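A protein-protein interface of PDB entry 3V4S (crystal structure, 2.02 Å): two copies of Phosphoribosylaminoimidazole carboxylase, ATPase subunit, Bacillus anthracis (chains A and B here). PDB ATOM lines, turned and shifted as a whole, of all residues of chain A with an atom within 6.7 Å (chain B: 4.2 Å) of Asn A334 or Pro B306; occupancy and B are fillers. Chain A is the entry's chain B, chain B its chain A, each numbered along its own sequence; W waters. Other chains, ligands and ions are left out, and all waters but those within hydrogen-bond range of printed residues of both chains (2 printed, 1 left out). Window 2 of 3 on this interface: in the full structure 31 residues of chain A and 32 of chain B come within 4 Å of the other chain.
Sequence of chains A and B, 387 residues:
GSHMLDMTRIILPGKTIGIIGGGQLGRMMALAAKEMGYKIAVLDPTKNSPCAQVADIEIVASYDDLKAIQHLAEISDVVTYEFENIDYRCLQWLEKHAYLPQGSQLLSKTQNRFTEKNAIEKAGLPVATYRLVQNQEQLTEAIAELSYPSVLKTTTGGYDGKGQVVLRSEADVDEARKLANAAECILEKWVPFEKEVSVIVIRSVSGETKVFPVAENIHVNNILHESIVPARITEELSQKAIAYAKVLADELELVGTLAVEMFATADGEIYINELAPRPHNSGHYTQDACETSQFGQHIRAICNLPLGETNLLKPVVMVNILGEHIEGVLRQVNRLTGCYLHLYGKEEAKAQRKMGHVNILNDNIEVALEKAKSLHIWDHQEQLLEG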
ATOM      1  N   VAL A 329       1.960  -3.185 -18.842  1.00  0.00           N
ATOM      2  CA  VAL A 329       3.296  -3.251 -18.244  1.00  0.00           C
ATOM      3  C   VAL A 329       4.383  -3.265 -19.316  1.00  0.00           C
ATOM      4  O   VAL A 329       5.313  -2.445 -19.279  1.00  0.00           O
ATOM      5  CB  VAL A 329       3.427  -4.469 -17.292  1.00  0.00           C
ATOM      6  CG1 VAL A 329       4.883  -4.672 -16.834  1.00  0.00           C
ATOM      7  CG2 VAL A 329       2.507  -4.268 -16.091  1.00  0.00           C
ATOM      8  N   LEU A 330       4.249  -4.176 -20.279  1.00  0.00           N
ATOM      9  CA  LEU A 330       5.256  -4.343 -21.333  1.00  0.00           C
ATOM     10  C   LEU A 330       5.359  -3.108 -22.221  1.00  0.00           C
ATOM     11  O   LEU A 330       6.463  -2.705 -22.609  1.00  0.00           O
ATOM     12  CB  LEU A 330       4.977  -5.596 -22.173  1.00  0.00           C
ATOM     13  CG  LEU A 330       5.043  -6.917 -21.407  1.00  0.00           C
ATOM     14  CD1 LEU A 330       4.533  -8.081 -22.256  1.00  0.00           C
ATOM     15  CD2 LEU A 330       6.456  -7.185 -20.903  1.00  0.00           C
ATOM     16  N   ARG A 331       4.213  -2.497 -22.518  1.00  0.00           N
ATOM     17  CA  ARG A 331       4.181  -1.252 -23.291  1.00  0.00           C
ATOM     18  C   ARG A 331       4.829  -0.102 -22.532  1.00  0.00           C
ATOM     19  O   ARG A 331       5.471   0.751 -23.130  1.00  0.00           O
ATOM     20  CB  ARG A 331       2.738  -0.892 -23.667  1.00  0.00           C
ATOM     21  CG  ARG A 331       2.593   0.303 -24.609  1.00  0.00           C
ATOM     22  CD  ARG A 331       1.201   0.417 -25.235  1.00  0.00           C
ATOM     23  NE  ARG A 331       0.110   0.241 -24.273  1.00  0.00           N
ATOM     24  CZ  ARG A 331      -0.661  -0.846 -24.195  1.00  0.00           C
ATOM     25  NH1 ARG A 331      -0.472  -1.866 -25.033  1.00  0.00           N
ATOM     26  NH2 ARG A 331      -1.629  -0.915 -23.284  1.00  0.00           N
ATOM     27  N   GLN A 332       4.646  -0.072 -21.216  1.00  0.00           N
ATOM     28  CA  GLN A 332       5.130   1.043 -20.409  1.00  0.00           C
ATOM     29  C   GLN A 332       6.469   0.745 -19.730  1.00  0.00           C
ATOM     30  O   GLN A 332       6.851   1.433 -18.766  1.00  0.00           O
ATOM     31  CB  GLN A 332       4.084   1.437 -19.362  1.00  0.00           C
ATOM     32  CG  GLN A 332       2.836   2.100 -19.935  1.00  0.00           C
ATOM     33  CD  GLN A 332       3.139   3.454 -20.545  1.00  0.00           C
ATOM     34  OE1 GLN A 332       3.006   4.485 -19.888  1.00  0.00           O
ATOM     35  NE2 GLN A 332       3.574   3.455 -21.796  1.00  0.00           N
ATOM     36  N   VAL A 333       7.182  -0.265 -20.233  1.00  0.00           N
ATOM     37  CA  VAL A 333       8.362  -0.774 -19.523  1.00  0.00           C
ATOM     38  C   VAL A 333       9.426   0.313 -19.352  1.00  0.00           C
ATOM     39  O   VAL A 333      10.095   0.368 -18.324  1.00  0.00           O
ATOM     40  CB  VAL A 333       8.936  -2.067 -20.154  1.00  0.00           C
ATOM     41  CG1 VAL A 333       9.902  -1.759 -21.292  1.00  0.00           C
ATOM     42  CG2 VAL A 333       9.645  -2.900 -19.097  1.00  0.00           C
ATOM     43  N   ASN A 334       9.535   1.195 -20.350  1.00  0.00           N
ATOM     44  CA  ASN A 334      10.504   2.289 -20.338  1.00  0.00           C
ATOM     45  C   ASN A 334      10.195   3.379 -19.308  1.00  0.00           C
ATOM     46  O   ASN A 334      11.003   4.284 -19.087  1.00  0.00           O
ATOM     47  CB  ASN A 334      10.678   2.875 -21.747  1.00  0.00           C
ATOM     48  CG  ASN A 334       9.361   3.291 -22.398  1.00  0.00           C
ATOM     49  OD1 ASN A 334       8.258   2.824 -22.047  1.00  0.00           O
ATOM     50  ND2 ASN A 334       9.479   4.158 -23.387  1.00  0.00           N
ATOM     51  N   ARG A 335       9.039   3.272 -18.654  1.00  0.00           N
ATOM     52  CA  ARG A 335       8.652   4.260 -17.643  1.00  0.00           C
ATOM     53  C   ARG A 335       8.765   3.766 -16.206  1.00  0.00           C
ATOM     54  O   ARG A 335       8.405   4.490 -15.273  1.00  0.00           O
ATOM     55  CB  ARG A 335       7.258   4.824 -17.948  1.00  0.00           C
ATOM     56  CG  ARG A 335       7.295   5.915 -19.018  1.00  0.00           C
ATOM     57  CD  ARG A 335       5.914   6.399 -19.400  1.00  0.00           C
ATOM     58  NE  ARG A 335       5.167   6.825 -18.223  1.00  0.00           N
ATOM     59  CZ  ARG A 335       3.884   7.169 -18.220  1.00  0.00           C
ATOM     60  NH1 ARG A 335       3.170   7.160 -19.339  1.00  0.00           N
ATOM     61  NH2 ARG A 335       3.316   7.534 -17.081  1.00  0.00           N
ATOM     62  N   LEU A 336       9.341   2.571 -16.032  1.00  0.00           N
ATOM     63  CA  LEU A 336       9.378   1.896 -14.729  1.00  0.00           C
ATOM     64  C   LEU A 336      10.562   2.298 -13.861  1.00  0.00           C
ATOM     65  O   LEU A 336      11.089   1.505 -13.062  1.00  0.00           O
ATOM     66  CB  LEU A 336       9.293   0.362 -14.898  1.00  0.00           C
ATOM     67  CG  LEU A 336       7.944  -0.156 -15.442  1.00  0.00           C
ATOM     68  CD1 LEU A 336       7.980  -1.666 -15.637  1.00  0.00           C
ATOM     69  CD2 LEU A 336       6.798   0.241 -14.515  1.00  0.00           C
ATOM     70  N   THR A 337      10.980   3.550 -13.987  1.00  0.00           N
ATOM     71  CA  THR A 337      12.019   4.056 -13.107  1.00  0.00           C
ATOM     72  C   THR A 337      11.490   4.026 -11.655  1.00  0.00           C
ATOM     73  O   THR A 337      10.320   4.302 -11.414  1.00  0.00           O
ATOM     74  CB  THR A 337      12.553   5.426 -13.601  1.00  0.00           C
ATOM     75  OG1 THR A 337      13.519   5.925 -12.677  1.00  0.00           O
ATOM     76  CG2 THR A 337      11.432   6.435 -13.739  1.00  0.00           C
ATOM     77  N   GLY A 338      12.333   3.607 -10.715  1.00  0.00           N
ATOM     78  CA  GLY A 338      11.942   3.413  -9.315  1.00  0.00           C
ATOM     79  C   GLY A 338      10.963   2.266  -9.051  1.00  0.00           C
ATOM     80  O   GLY A 338      10.392   2.157  -7.967  1.00  0.00           O
ATOM     81  N   CYS A 339      10.761   1.419 -10.046  1.00  0.00           N
ATOM     82  CA  CYS A 339       9.784   0.346  -9.963  1.00  0.00           C
ATOM     83  C   CYS A 339      10.528  -0.966 -10.181  1.00  0.00           C
ATOM     84  O   CYS A 339      11.334  -1.083 -11.117  1.00  0.00           O
ATOM     85  CB  CYS A 339       8.696   0.526 -11.023  1.00  0.00           C
ATOM     86  SG  CYS A 339       7.817   2.105 -10.951  1.00  0.00           S
ATOM     87  N   GLU B 208      21.668   5.575 -20.085  1.00  0.00           N
ATOM     88  CA  GLU B 208      21.398   5.872 -18.671  1.00  0.00           C
ATOM     89  C   GLU B 208      22.534   5.317 -17.783  1.00  0.00           C
ATOM     90  O   GLU B 208      22.994   4.212 -18.020  1.00  0.00           O
ATOM     91  CB  GLU B 208      20.051   5.291 -18.230  1.00  0.00           C
ATOM     92  CG  GLU B 208      19.736   5.598 -16.778  1.00  0.00           C
ATOM     93  CD  GLU B 208      18.421   5.016 -16.294  1.00  0.00           C
ATOM     94  OE1 GLU B 208      17.953   5.475 -15.233  1.00  0.00           O
ATOM     95  OE2 GLU B 208      17.855   4.119 -16.952  1.00  0.00           O
ATOM     96  N   ARG B 300      19.108  -5.239 -16.576  1.00  0.00           N
ATOM     97  CA  ARG B 300      18.398  -4.057 -17.061  1.00  0.00           C
ATOM     98  C   ARG B 300      19.217  -3.298 -18.102  1.00  0.00           C
ATOM     99  O   ARG B 300      18.667  -2.830 -19.114  1.00  0.00           O
ATOM    100  CB  ARG B 300      18.038  -3.129 -15.911  1.00  0.00           C
ATOM    101  CG  ARG B 300      16.983  -3.692 -14.970  1.00  0.00           C
ATOM    102  CD  ARG B 300      16.928  -2.891 -13.671  1.00  0.00           C
ATOM    103  NE  ARG B 300      15.716  -3.194 -12.905  1.00  0.00           N
ATOM    104  CZ  ARG B 300      15.557  -4.270 -12.130  1.00  0.00           C
ATOM    105  NH1 ARG B 300      16.557  -5.144 -11.978  1.00  0.00           N
ATOM    106  NH2 ARG B 300      14.397  -4.461 -11.482  1.00  0.00           N
ATOM    107  N   LEU B 305      16.255  -1.688 -20.082  1.00  0.00           N
ATOM    108  CA  LEU B 305      15.182  -1.299 -19.181  1.00  0.00           C
ATOM    109  C   LEU B 305      15.682  -0.122 -18.360  1.00  0.00           C
ATOM    110  O   LEU B 305      16.905   0.090 -18.263  1.00  0.00           O
ATOM    111  CB  LEU B 305      14.797  -2.463 -18.250  1.00  0.00           C
ATOM    112  CG  LEU B 305      14.484  -3.807 -18.892  1.00  0.00           C
ATOM    113  CD1 LEU B 305      14.105  -4.846 -17.834  1.00  0.00           C
ATOM    114  CD2 LEU B 305      13.386  -3.695 -19.949  1.00  0.00           C
ATOM    115  N   PRO B 306      14.763   0.640 -17.737  1.00  0.00           N
ATOM    116  CA  PRO B 306      15.212   1.697 -16.821  1.00  0.00           C
ATOM    117  C   PRO B 306      16.057   1.049 -15.713  1.00  0.00           C
ATOM    118  O   PRO B 306      15.707  -0.040 -15.223  1.00  0.00           O
ATOM    119  CB  PRO B 306      13.899   2.204 -16.218  1.00  0.00           C
ATOM    120  CG  PRO B 306      12.863   1.823 -17.218  1.00  0.00           C
ATOM    121  CD  PRO B 306      13.303   0.460 -17.652  1.00  0.00           C
ATOM    122  N   LEU B 307      17.146   1.696 -15.316  1.00  0.00           N
ATOM    123  CA  LEU B 307      18.018   1.106 -14.315  1.00  0.00           C
ATOM    124  C   LEU B 307      17.401   1.356 -12.939  1.00  0.00           C
ATOM    125  O   LEU B 307      16.677   2.345 -12.740  1.00  0.00           O
ATOM    126  CB  LEU B 307      19.416   1.723 -14.386  1.00  0.00           C
ATOM    127  CG  LEU B 307      20.218   1.582 -15.680  1.00  0.00           C
ATOM    128  CD1 LEU B 307      21.595   2.242 -15.520  1.00  0.00           C
ATOM    129  CD2 LEU B 307      20.365   0.120 -16.097  1.00  0.00           C
ATOM    130  N   GLY B 308      17.677   0.449 -12.007  1.00  0.00           N
ATOM    131  CA  GLY B 308      17.249   0.618 -10.627  1.00  0.00           C
ATOM    132  C   GLY B 308      18.168   1.579  -9.888  1.00  0.00           C
ATOM    133  O   GLY B 308      19.198   1.989 -10.406  1.00  0.00           O
HETATM  134  O   HOH W   1      15.849   4.617 -13.967  1.00  0.00           O
HETATM  135  O   HOH W   2      15.196   3.376 -10.735  1.00  0.00           O
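The backbone carbonyl oxygen (O) of Arg B300 is in hydrogen-bond range of the backbone NH (N) of Leu B305 (2.8 Å). SG of Cys A339 is in hydrogen-bond range of O of Thr A337 (3.4 Å).
Among the printed residues, merely in contact across the chains: Val A333 with Leu B305 (3.9 Å), Val A333 with Pro B306 (3.3 Å), Asn A334 with Pro B306 (3.6 Å), Leu A336 with Pro B306 (3.8 Å) and Thr A337 with Pro B306 (3.9 Å).
Asn A334 touches one residue of chain B. Of chain A, only Val A333 (3.3 Å), Asn A334 (3.6 Å), Leu A336 (3.8 Å) and Thr A337 (3.9 Å) come within 4 Å of Pro B306. Of the printed residues of chain B, Leu A336 touches Pro B306. Of the printed residues of chain A, Leu B305 touches Val A333. The nearest printed residue of chain B that does not touch Asn A334 is Leu B305 (6.0 Å). The nearest residue of chain A that does not touch Pro B306 is Arg A335 (4.3 Å). The nearest printed residue of chain A that does not touch Leu B305 is Asn A334 (6.0 Å).
Of the 6 printed residues of chain B, 2 touch a printed residue of chain A. Hydrophobic or aromatic side chains of chain B that line the printed part of chain A: Leu B305 and Pro B306. Along chain B the printed residues that touch a printed residue of chain A span positions 305 to 306. Of the 11 printed residues of chain A, 4 touch a printed residue of chain B. Printed residues of chain A that touch a printed residue of chain B: Val A333, Asn A334, Leu A336 and Thr A337. Hydrophobic or aromatic side chains of chain A that line the printed part of chain B: Val A333.
No position is printed for both chains. Of the 5 pairs that touch across the chains among the printed residues, none has its exchanged pair printed and touching as well.
Water W1 lies within hydrogen-bond range of the side-chain carboxylate (OE1) of Glu B208 (2.6 Å), the backbone carbonyl oxygen (O) of Leu B307 (2.7 Å) and the side-chain hydroxyl (OG1) of Thr A337 (3.0 Å). Water W2 lies within hydrogen-bond range of O of Leu B307 (2.7 Å) and N of Gly A338 (2.9 Å).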
